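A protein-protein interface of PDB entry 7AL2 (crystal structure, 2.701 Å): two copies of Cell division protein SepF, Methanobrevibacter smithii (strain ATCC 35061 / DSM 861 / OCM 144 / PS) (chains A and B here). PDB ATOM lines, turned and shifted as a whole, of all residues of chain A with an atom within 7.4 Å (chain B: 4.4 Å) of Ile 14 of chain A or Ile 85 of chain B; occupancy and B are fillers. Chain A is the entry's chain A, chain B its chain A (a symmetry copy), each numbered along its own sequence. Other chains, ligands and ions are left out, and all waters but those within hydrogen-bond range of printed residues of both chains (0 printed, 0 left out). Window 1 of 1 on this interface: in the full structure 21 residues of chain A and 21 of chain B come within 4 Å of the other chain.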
ATOM      1  N   TYR A  12      -7.391  -4.869  10.866  1.00  0.00           N
ATOM      2  CA  TYR A  12      -8.118  -3.794  10.162  1.00  0.00           C
ATOM      3  C   TYR A  12      -9.502  -3.424  10.824  1.00  0.00           C
ATOM      4  O   TYR A  12      -9.744  -3.715  12.001  1.00  0.00           O
ATOM      5  CB  TYR A  12      -8.280  -4.106   8.626  1.00  0.00           C
ATOM      6  N   GLU A  13     -10.361  -2.715  10.065  1.00  0.00           N
ATOM      7  CA  GLU A  13     -11.690  -2.314  10.480  1.00  0.00           C
ATOM      8  C   GLU A  13     -12.656  -2.633   9.354  1.00  0.00           C
ATOM      9  O   GLU A  13     -12.265  -2.700   8.195  1.00  0.00           O
ATOM     10  CB  GLU A  13     -11.729  -0.800  10.715  1.00  0.00           C
ATOM     11  CG  GLU A  13     -10.707  -0.306  11.714  1.00  0.00           C
ATOM     12  CD  GLU A  13     -10.397   1.163  11.538  1.00  0.00           C
ATOM     13  OE1 GLU A  13      -9.692   1.513  10.561  1.00  0.00           O
ATOM     14  OE2 GLU A  13     -10.862   1.965  12.381  1.00  0.00           O
ATOM     15  N   ILE A  14     -13.922  -2.823   9.692  1.00  0.00           N
ATOM     16  CA  ILE A  14     -14.993  -3.009   8.720  1.00  0.00           C
ATOM     17  C   ILE A  14     -15.884  -1.805   8.981  1.00  0.00           C
ATOM     18  O   ILE A  14     -16.344  -1.628  10.106  1.00  0.00           O
ATOM     19  CB  ILE A  14     -15.782  -4.338   8.899  1.00  0.00           C
ATOM     20  CG1 ILE A  14     -14.871  -5.583   8.708  1.00  0.00           C
ATOM     21  CG2 ILE A  14     -16.956  -4.374   7.947  1.00  0.00           C
ATOM     22  CD1 ILE A  14     -15.424  -6.821   9.228  1.00  0.00           C
ATOM     23  N   MET A  15     -16.060  -0.935   7.987  1.00  0.00           N
ATOM     24  CA  MET A  15     -16.874   0.262   8.149  1.00  0.00           C
ATOM     25  C   MET A  15     -18.310  -0.011   7.767  1.00  0.00           C
ATOM     26  O   MET A  15     -18.572  -0.810   6.887  1.00  0.00           O
ATOM     27  CB  MET A  15     -16.308   1.426   7.329  1.00  0.00           C
ATOM     28  CG  MET A  15     -14.806   1.511   7.376  1.00  0.00           C
ATOM     29  SD  MET A  15     -14.127   1.726   9.041  1.00  0.00           S
ATOM     30  CE  MET A  15     -14.671   3.315   9.390  1.00  0.00           C
ATOM     31  N   LEU A  16     -19.247   0.654   8.424  1.00  0.00           N
ATOM     32  CA  LEU A  16     -20.673   0.445   8.185  1.00  0.00           C
ATOM     33  C   LEU A  16     -21.298   1.799   7.850  1.00  0.00           C
ATOM     34  O   LEU A  16     -21.118   2.740   8.605  1.00  0.00           O
ATOM     35  CB  LEU A  16     -21.294  -0.192   9.445  1.00  0.00           C
ATOM     36  CG  LEU A  16     -20.589  -1.481   9.908  1.00  0.00           C
ATOM     37  CD1 LEU A  16     -20.289  -1.457  11.377  1.00  0.00           C
ATOM     38  CD2 LEU A  16     -21.348  -2.694   9.518  1.00  0.00           C
ATOM     39  N   GLN A  31     -11.978   4.274   1.869  1.00  0.00           N
ATOM     40  CA  GLN A  31     -11.778   3.214   2.863  1.00  0.00           C
ATOM     41  C   GLN A  31     -11.257   1.955   2.151  1.00  0.00           C
ATOM     42  O   GLN A  31     -10.261   1.358   2.571  1.00  0.00           O
ATOM     43  CB  GLN A  31     -13.078   2.907   3.639  1.00  0.00           C
ATOM     44  CG  GLN A  31     -13.496   3.998   4.601  1.00  0.00           C
ATOM     45  CD  GLN A  31     -12.565   4.102   5.778  1.00  0.00           C
ATOM     46  OE1 GLN A  31     -12.084   3.118   6.312  1.00  0.00           O
ATOM     47  NE2 GLN A  31     -12.290   5.303   6.230  1.00  0.00           N
ATOM     48  N   ASN A  37      -9.843  -1.140   3.998  1.00  0.00           N
ATOM     49  CA  ASN A  37     -10.839  -1.588   4.946  1.00  0.00           C
ATOM     50  C   ASN A  37     -12.084  -2.027   4.188  1.00  0.00           C
ATOM     51  O   ASN A  37     -12.583  -1.279   3.347  1.00  0.00           O
ATOM     52  CB  ASN A  37     -11.250  -0.439   5.866  1.00  0.00           C
ATOM     53  CG  ASN A  37     -10.238  -0.084   6.908  1.00  0.00           C
ATOM     54  OD1 ASN A  37      -9.421  -0.915   7.314  1.00  0.00           O
ATOM     55  ND2 ASN A  37     -10.287   1.152   7.388  1.00  0.00           N
ATOM     56  N   PRO A  38     -12.656  -3.199   4.529  1.00  0.00           N
ATOM     57  CA  PRO A  38     -13.946  -3.572   3.931  1.00  0.00           C
ATOM     58  C   PRO A  38     -15.049  -2.595   4.382  1.00  0.00           C
ATOM     59  O   PRO A  38     -14.960  -1.999   5.456  1.00  0.00           O
ATOM     60  CB  PRO A  38     -14.209  -4.983   4.476  1.00  0.00           C
ATOM     61  CG  PRO A  38     -12.929  -5.429   5.108  1.00  0.00           C
ATOM     62  CD  PRO A  38     -12.209  -4.190   5.525  1.00  0.00           C
ATOM     63  N   VAL A  39     -16.065  -2.389   3.540  1.00  0.00           N
ATOM     64  CA  VAL A  39     -17.175  -1.495   3.873  1.00  0.00           C
ATOM     65  C   VAL A  39     -18.470  -2.244   3.670  1.00  0.00           C
ATOM     66  O   VAL A  39     -18.676  -2.822   2.599  1.00  0.00           O
ATOM     67  CB  VAL A  39     -17.198  -0.204   3.001  1.00  0.00           C
ATOM     68  CG1 VAL A  39     -18.288   0.757   3.475  1.00  0.00           C
ATOM     69  CG2 VAL A  39     -15.840   0.491   2.970  1.00  0.00           C
ATOM     70  N   ILE A  40     -19.342  -2.238   4.678  1.00  0.00           N
ATOM     71  CA  ILE A  40     -20.686  -2.792   4.575  1.00  0.00           C
ATOM     72  C   ILE A  40     -21.553  -1.567   4.379  1.00  0.00           C
ATOM     73  O   ILE A  40     -21.576  -0.694   5.252  1.00  0.00           O
ATOM     74  CB  ILE A  40     -21.121  -3.589   5.822  1.00  0.00           C
ATOM     75  CG1 ILE A  40     -20.160  -4.767   6.089  1.00  0.00           C
ATOM     76  CG2 ILE A  40     -22.565  -4.050   5.658  1.00  0.00           C
ATOM     77  CD1 ILE A  40     -20.505  -5.660   7.292  1.00  0.00           C
ATOM     78  N   LEU A  75     -25.595  -8.833   0.163  1.00  0.00           N
ATOM     79  CA  LEU A  75     -25.905  -9.576   1.362  1.00  0.00           C
ATOM     80  C   LEU A  75     -27.404  -9.636   1.639  1.00  0.00           C
ATOM     81  O   LEU A  75     -27.875 -10.611   2.231  1.00  0.00           O
ATOM     82  CB  LEU A  75     -25.186  -8.916   2.560  1.00  0.00           C
ATOM     83  CG  LEU A  75     -23.671  -9.048   2.608  1.00  0.00           C
ATOM     84  CD1 LEU A  75     -23.098  -8.193   3.708  1.00  0.00           C
ATOM     85  CD2 LEU A  75     -23.246 -10.508   2.760  1.00  0.00           C
ATOM     86  N   ILE A  85     -21.408  -5.637   0.548  1.00  0.00           N
ATOM     87  CA  ILE A  85     -20.120  -5.631   1.225  1.00  0.00           C
ATOM     88  C   ILE A  85     -19.038  -5.497   0.165  1.00  0.00           C
ATOM     89  O   ILE A  85     -19.062  -6.203  -0.847  1.00  0.00           O
ATOM     90  CB  ILE A  85     -19.839  -6.743   2.278  1.00  0.00           C
ATOM     91  CG1 ILE A  85     -18.472  -6.485   2.965  1.00  0.00           C
ATOM     92  CG2 ILE A  85     -19.916  -8.153   1.678  1.00  0.00           C
ATOM     93  CD1 ILE A  85     -18.066  -7.431   4.106  1.00  0.00           C
ATOM     94  N   ILE A  86     -18.135  -4.538   0.365  1.00  0.00           N
ATOM     95  CA  ILE A  86     -17.025  -4.349  -0.547  1.00  0.00           C
ATOM     96  C   ILE A  86     -15.742  -4.700   0.214  1.00  0.00           C
ATOM     97  O   ILE A  86     -15.424  -4.048   1.198  1.00  0.00           O
ATOM     98  CB  ILE A  86     -16.951  -2.905  -1.085  1.00  0.00           C
ATOM     99  CG1 ILE A  86     -18.311  -2.412  -1.591  1.00  0.00           C
ATOM    100  CG2 ILE A  86     -15.859  -2.783  -2.145  1.00  0.00           C
ATOM    101  CD1 ILE A  86     -18.328  -0.910  -1.989  1.00  0.00           C
ATOM    102  N   VAL A  91      -8.416  -8.795   1.382  1.00  0.00           N
ATOM    103  CA  VAL A  91      -9.409  -9.392   2.250  1.00  0.00           C
ATOM    104  C   VAL A  91     -10.289 -10.238   1.341  1.00  0.00           C
ATOM    105  O   VAL A  91     -10.922  -9.727   0.421  1.00  0.00           O
ATOM    106  CB  VAL A  91     -10.223  -8.363   3.075  1.00  0.00           C
ATOM    107  CG1 VAL A  91     -11.285  -9.057   3.919  1.00  0.00           C
ATOM    108  CG2 VAL A  91      -9.310  -7.503   3.949  1.00  0.00           C
ATOM    109  N   PRO B  38     -13.472 -12.561  10.715  1.00  0.00           N
ATOM    110  CA  PRO B  38     -14.897 -12.237  10.881  1.00  0.00           C
ATOM    111  C   PRO B  38     -15.770 -13.249  10.115  1.00  0.00           C
ATOM    112  O   PRO B  38     -15.332 -13.836   9.126  1.00  0.00           O
ATOM    113  CB  PRO B  38     -15.027 -10.832  10.274  1.00  0.00           C
ATOM    114  CG  PRO B  38     -13.630 -10.339  10.068  1.00  0.00           C
ATOM    115  CD  PRO B  38     -12.774 -11.549   9.902  1.00  0.00           C
ATOM    116  N   VAL B  39     -16.990 -13.495  10.601  1.00  0.00           N
ATOM    117  CA  VAL B  39     -17.909 -14.425   9.946  1.00  0.00           C
ATOM    118  C   VAL B  39     -19.229 -13.724   9.732  1.00  0.00           C
ATOM    119  O   VAL B  39     -19.778 -13.159  10.683  1.00  0.00           O
ATOM    120  CB  VAL B  39     -18.156 -15.721  10.774  1.00  0.00           C
ATOM    121  CG1 VAL B  39     -19.012 -16.718   9.990  1.00  0.00           C
ATOM    122  CG2 VAL B  39     -16.852 -16.368  11.230  1.00  0.00           C
ATOM    123  N   ILE B  40     -19.744 -13.754   8.504  1.00  0.00           N
ATOM    124  CA  ILE B  40     -21.072 -13.248   8.181  1.00  0.00           C
ATOM    125  C   ILE B  40     -21.914 -14.504   8.105  1.00  0.00           C
ATOM    126  O   ILE B  40     -21.633 -15.372   7.272  1.00  0.00           O
ATOM    127  CB  ILE B  40     -21.127 -12.460   6.856  1.00  0.00           C
ATOM    128  CG1 ILE B  40     -20.171 -11.249   6.894  1.00  0.00           C
ATOM    129  CG2 ILE B  40     -22.565 -12.052   6.561  1.00  0.00           C
ATOM    130  CD1 ILE B  40     -20.157 -10.361   5.638  1.00  0.00           C
ATOM    131  N   GLU B  71     -17.244  -8.701  18.634  1.00  0.00           N
ATOM    132  CA  GLU B  71     -18.408  -7.837  18.457  1.00  0.00           C
ATOM    133  C   GLU B  71     -19.383  -8.603  17.553  1.00  0.00           C
ATOM    134  O   GLU B  71     -18.956  -9.367  16.684  1.00  0.00           O
ATOM    135  CB  GLU B  71     -18.055  -6.477  17.825  1.00  0.00           C
ATOM    136  CG  GLU B  71     -16.961  -5.692  18.534  1.00  0.00           C
ATOM    137  CD  GLU B  71     -16.475  -4.478  17.759  1.00  0.00           C
ATOM    138  OE1 GLU B  71     -16.506  -4.530  16.511  1.00  0.00           O
ATOM    139  OE2 GLU B  71     -16.055  -3.476  18.389  1.00  0.00           O
ATOM    140  N   ALA B  72     -20.685  -8.433  17.763  1.00  0.00           N
ATOM    141  CA  ALA B  72     -21.702  -9.075  16.925  1.00  0.00           C
ATOM    142  C   ALA B  72     -22.752  -8.035  16.532  1.00  0.00           C
ATOM    143  O   ALA B  72     -23.218  -7.263  17.375  1.00  0.00           O
ATOM    144  CB  ALA B  72     -22.343 -10.243  17.646  1.00  0.00           C
ATOM    145  N   LEU B  73     -23.101  -7.990  15.255  1.00  0.00           N
ATOM    146  CA  LEU B  73     -24.041  -7.002  14.753  1.00  0.00           C
ATOM    147  C   LEU B  73     -25.094  -7.654  13.911  1.00  0.00           C
ATOM    148  O   LEU B  73     -24.769  -8.507  13.094  1.00  0.00           O
ATOM    149  CB  LEU B  73     -23.267  -6.007  13.871  1.00  0.00           C
ATOM    150  CG  LEU B  73     -23.442  -4.519  14.135  1.00  0.00           C
ATOM    151  CD1 LEU B  73     -23.188  -4.176  15.606  1.00  0.00           C
ATOM    152  CD2 LEU B  73     -22.534  -3.693  13.219  1.00  0.00           C
ATOM    153  N   LEU B  75     -27.317  -7.408  10.817  1.00  0.00           N
ATOM    154  CA  LEU B  75     -27.266  -6.670   9.576  1.00  0.00           C
ATOM    155  C   LEU B  75     -28.605  -6.661   8.847  1.00  0.00           C
ATOM    156  O   LEU B  75     -28.903  -5.699   8.133  1.00  0.00           O
ATOM    157  CB  LEU B  75     -26.188  -7.298   8.664  1.00  0.00           C
ATOM    158  CG  LEU B  75     -24.738  -7.112   9.089  1.00  0.00           C
ATOM    159  CD1 LEU B  75     -23.822  -7.941   8.225  1.00  0.00           C
ATOM    160  CD2 LEU B  75     -24.338  -5.637   9.068  1.00  0.00           C
ATOM    161  N   ILE B  84     -26.152 -12.016  10.606  1.00  0.00           N
ATOM    162  CA  ILE B  84     -25.334 -11.529  11.703  1.00  0.00           C
ATOM    163  C   ILE B  84     -23.859 -11.437  11.254  1.00  0.00           C
ATOM    164  O   ILE B  84     -23.407 -12.266  10.468  1.00  0.00           O
ATOM    165  CB  ILE B  84     -25.483 -12.530  12.911  1.00  0.00           C
ATOM    166  CG1 ILE B  84     -26.919 -12.584  13.440  1.00  0.00           C
ATOM    167  CG2 ILE B  84     -24.474 -12.280  14.042  1.00  0.00           C
ATOM    168  CD1 ILE B  84     -27.356 -11.382  14.196  1.00  0.00           C
ATOM    169  N   ILE B  85     -23.108 -10.453  11.769  1.00  0.00           N
ATOM    170  CA  ILE B  85     -21.675 -10.411  11.525  1.00  0.00           C
ATOM    171  C   ILE B  85     -20.972 -10.512  12.870  1.00  0.00           C
ATOM    172  O   ILE B  85     -21.333  -9.813  13.820  1.00  0.00           O
ATOM    173  CB  ILE B  85     -21.119  -9.283  10.605  1.00  0.00           C
ATOM    174  CG1 ILE B  85     -19.598  -9.490  10.378  1.00  0.00           C
ATOM    175  CG2 ILE B  85     -21.428  -7.880  11.143  1.00  0.00           C
ATOM    176  CD1 ILE B  85     -18.892  -8.524   9.414  1.00  0.00           C
ATOM    177  N   ILE B  86     -20.017 -11.438  12.965  1.00  0.00           N
ATOM    178  CA  ILE B  86     -19.239 -11.593  14.178  1.00  0.00           C
ATOM    179  C   ILE B  86     -17.796 -11.193  13.851  1.00  0.00           C
ATOM    180  O   ILE B  86     -17.166 -11.828  13.018  1.00  0.00           O
ATOM    181  CB  ILE B  86     -19.285 -13.036  14.720  1.00  0.00           C
ATOM    182  CG1 ILE B  86     -20.717 -13.580  14.782  1.00  0.00           C
ATOM    183  CG2 ILE B  86     -18.574 -13.126  16.067  1.00  0.00           C
ATOM    184  CD1 ILE B  86     -20.804 -15.084  15.162  1.00  0.00           C
ATOM    185  N   ALA B  87     -17.282 -10.148  14.500  1.00  0.00           N
ATOM    186  CA  ALA B  87     -15.905  -9.726  14.304  1.00  0.00           C
ATOM    187  C   ALA B  87     -15.112 -10.141  15.525  1.00  0.00           C
ATOM    188  O   ALA B  87     -15.550  -9.914  16.656  1.00  0.00           O
ATOM    189  CB  ALA B  87     -15.830  -8.213  14.130  1.00  0.00           C
ATOM    190  N   VAL B  91     -10.619  -6.837  14.992  1.00  0.00           N
ATOM    191  CA  VAL B  91     -11.313  -6.270  13.855  1.00  0.00           C
ATOM    192  C   VAL B  91     -12.460  -5.460  14.441  1.00  0.00           C
ATOM    193  O   VAL B  91     -13.331  -5.999  15.122  1.00  0.00           O
ATOM    194  CB  VAL B  91     -11.794  -7.322  12.824  1.00  0.00           C
ATOM    195  CG1 VAL B  91     -12.566  -6.662  11.688  1.00  0.00           C
ATOM    196  CG2 VAL B  91     -10.626  -8.145  12.282  1.00  0.00           C
ATOM    197  N   SER B  92     -12.421  -4.158  14.246  1.00  0.00           N
ATOM    198  CA  SER B  92     -13.462  -3.265  14.740  1.00  0.00           C
ATOM    199  C   SER B  92     -14.570  -3.075  13.724  1.00  0.00           C
ATOM    200  O   SER B  92     -14.291  -2.859  12.545  1.00  0.00           O
ATOM    201  CB  SER B  92     -12.869  -1.899  15.037  1.00  0.00           C
ATOM    202  OG  SER B  92     -11.791  -2.053  15.941  1.00  0.00           O
ATOM    203  N   LEU B  93     -15.830  -3.116  14.193  1.00  0.00           N
ATOM    204  CA  LEU B  93     -17.000  -2.798  13.384  1.00  0.00           C
ATOM    205  C   LEU B  93     -17.238  -1.341  13.702  1.00  0.00           C
ATOM    206  O   LEU B  93     -17.482  -0.988  14.853  1.00  0.00           O
ATOM    207  CB  LEU B  93     -18.208  -3.652  13.750  1.00  0.00           C
ATOM    208  CG  LEU B  93     -18.019  -5.138  13.467  1.00  0.00           C
ATOM    209  CD1 LEU B  93     -19.109  -5.971  14.109  1.00  0.00           C
ATOM    210  CD2 LEU B  93     -17.889  -5.407  11.982  1.00  0.00           C
ATOM    211  N   VAL B  94     -17.008  -0.484  12.724  1.00  0.00           N
ATOM    212  CA  VAL B  94     -17.115   0.937  12.926  1.00  0.00           C
ATOM    213  C   VAL B  94     -18.300   1.512  12.181  1.00  0.00           C
ATOM    214  O   VAL B  94     -18.303   1.566  10.949  1.00  0.00           O
ATOM    215  CB  VAL B  94     -15.796   1.648  12.573  1.00  0.00           C
ATOM    216  CG1 VAL B  94     -15.929   3.158  12.747  1.00  0.00           C
ATOM    217  CG2 VAL B  94     -14.648   1.106  13.407  1.00  0.00           C
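Tyr 12 of chain A touches Val 91 of chain B (O to CA, 3.5 Å).
Tyr 12 of chain A touches Ser 92 of chain B.
Glu 13 of chain A touches Ser 92 of chain B (CA to O, 3.4 Å).
CD1 of Ile 14 of chain A touches CD1 of Ile 85 of chain B, 3.9 Å away.
Ile 14 of chain A touches Val 91 of chain B.
Ile 14 of chain A touches Leu 93 of chain B (O to CA, 3.5 Å).
Met 15 of chain A touches Val 94 of chain B (CA to O, 3.4 Å).
Leu 73 of chain B touches Leu 16 of chain A (CD2 to CD1, 3.7 Å).
Ile 40 of chain A touches Ile 85 of chain B.
CD1 of Ile 85 of chain A touches CD1 of Ile 40 of chain B, at 3.9 Å.
Of the 15 printed residues of chain B, 7 touch a printed residue of chain A.
Hydrophobic or aromatic side chains of chain B that line the printed part of chain A: Ile 40, Leu 73, Ile 85, Val 91, Leu 93 and Val 94.
Along chain B the printed residues that touch a printed residue of chain A span positions 40 to 94.
Along chain A the printed residues that touch a printed residue of chain B span positions 12 to 85.
Among the printed residues, 14 pairs touch across the chains.
Among the printed residues, no Asp or Glu carboxylate lies within 4 Å of a Lys or Arg side-chain nitrogen of the other chain.
Ile 14 of chain A touches five residues of chain B.
Of the printed residues of chain B, Met 15 of chain A touches Val 94 (3.4 Å).
Of the printed residues of chain B, Leu 16 of chain A touches Leu 73 (3.7 Å), Leu 93 (3.8 Å) and Val 94 (2.8 Å).
Ala 72 of chain B touches none of the printed residues of chain A.
Ile 85 of chain B touches just these residues of chain A: Ile 14 and Ile 40.
The nearest residue of chain B that does not touch Ile 14 of chain A is Pro 38 of chain B (4.04 Å).
The backbone carbonyl oxygen (O) of Ile 14 of chain A lies within hydrogen-bond range of the backbone NH (N) of Val 94 of chain B (2.9 Å).
The backbone carbonyl oxygen (O) of Val 94 of chain B sits at hydrogen-bond distance from the backbone NH (N) of Leu 16 of chain A (2.8 Å).
O of Ser 92 of chain B sits at hydrogen-bond distance from N of Ile 14 of chain A, at 2.9 Å.
The backbone NH of Ile 85 of chain B lies within hydrogen-bond range of the backbone carbonyl oxygen of Leu 73 of chain B (2.9 Å).
The backbone carbonyl oxygen of Pro 38 of chain A sits at hydrogen-bond distance from the backbone NH of Met 15 of chain A.
The backbone NH (N) of Ile 40 of chain A lies within hydrogen-bond range of the backbone carbonyl oxygen (O) of Met 15 of chain A.
OE1 of Glu 71 of chain B lies within hydrogen-bond range of N of Leu 93 of chain B, at 2.8 Å.
The side-chain amide oxygen (OE1) of Gln 31 of chain A sits close to the side-chain sulfur (SD) of Met 15 of chain A, 3.7 Å away.
The side-chain carboxylate (OE1) of Glu 13 of chain A is in hydrogen-bond range of the side-chain amide nitrogen (ND2) of Asn 37 of chain A (3.2 Å).
Ile 40 of chain A touches Ile 85 of chain B, and with the chains exchanged Ile 85 of chain A touches Ile 40 of chain B.
Of the 14 pairs that touch across the chains among the printed residues, 2 have their exchanged pair printed and touching as well.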
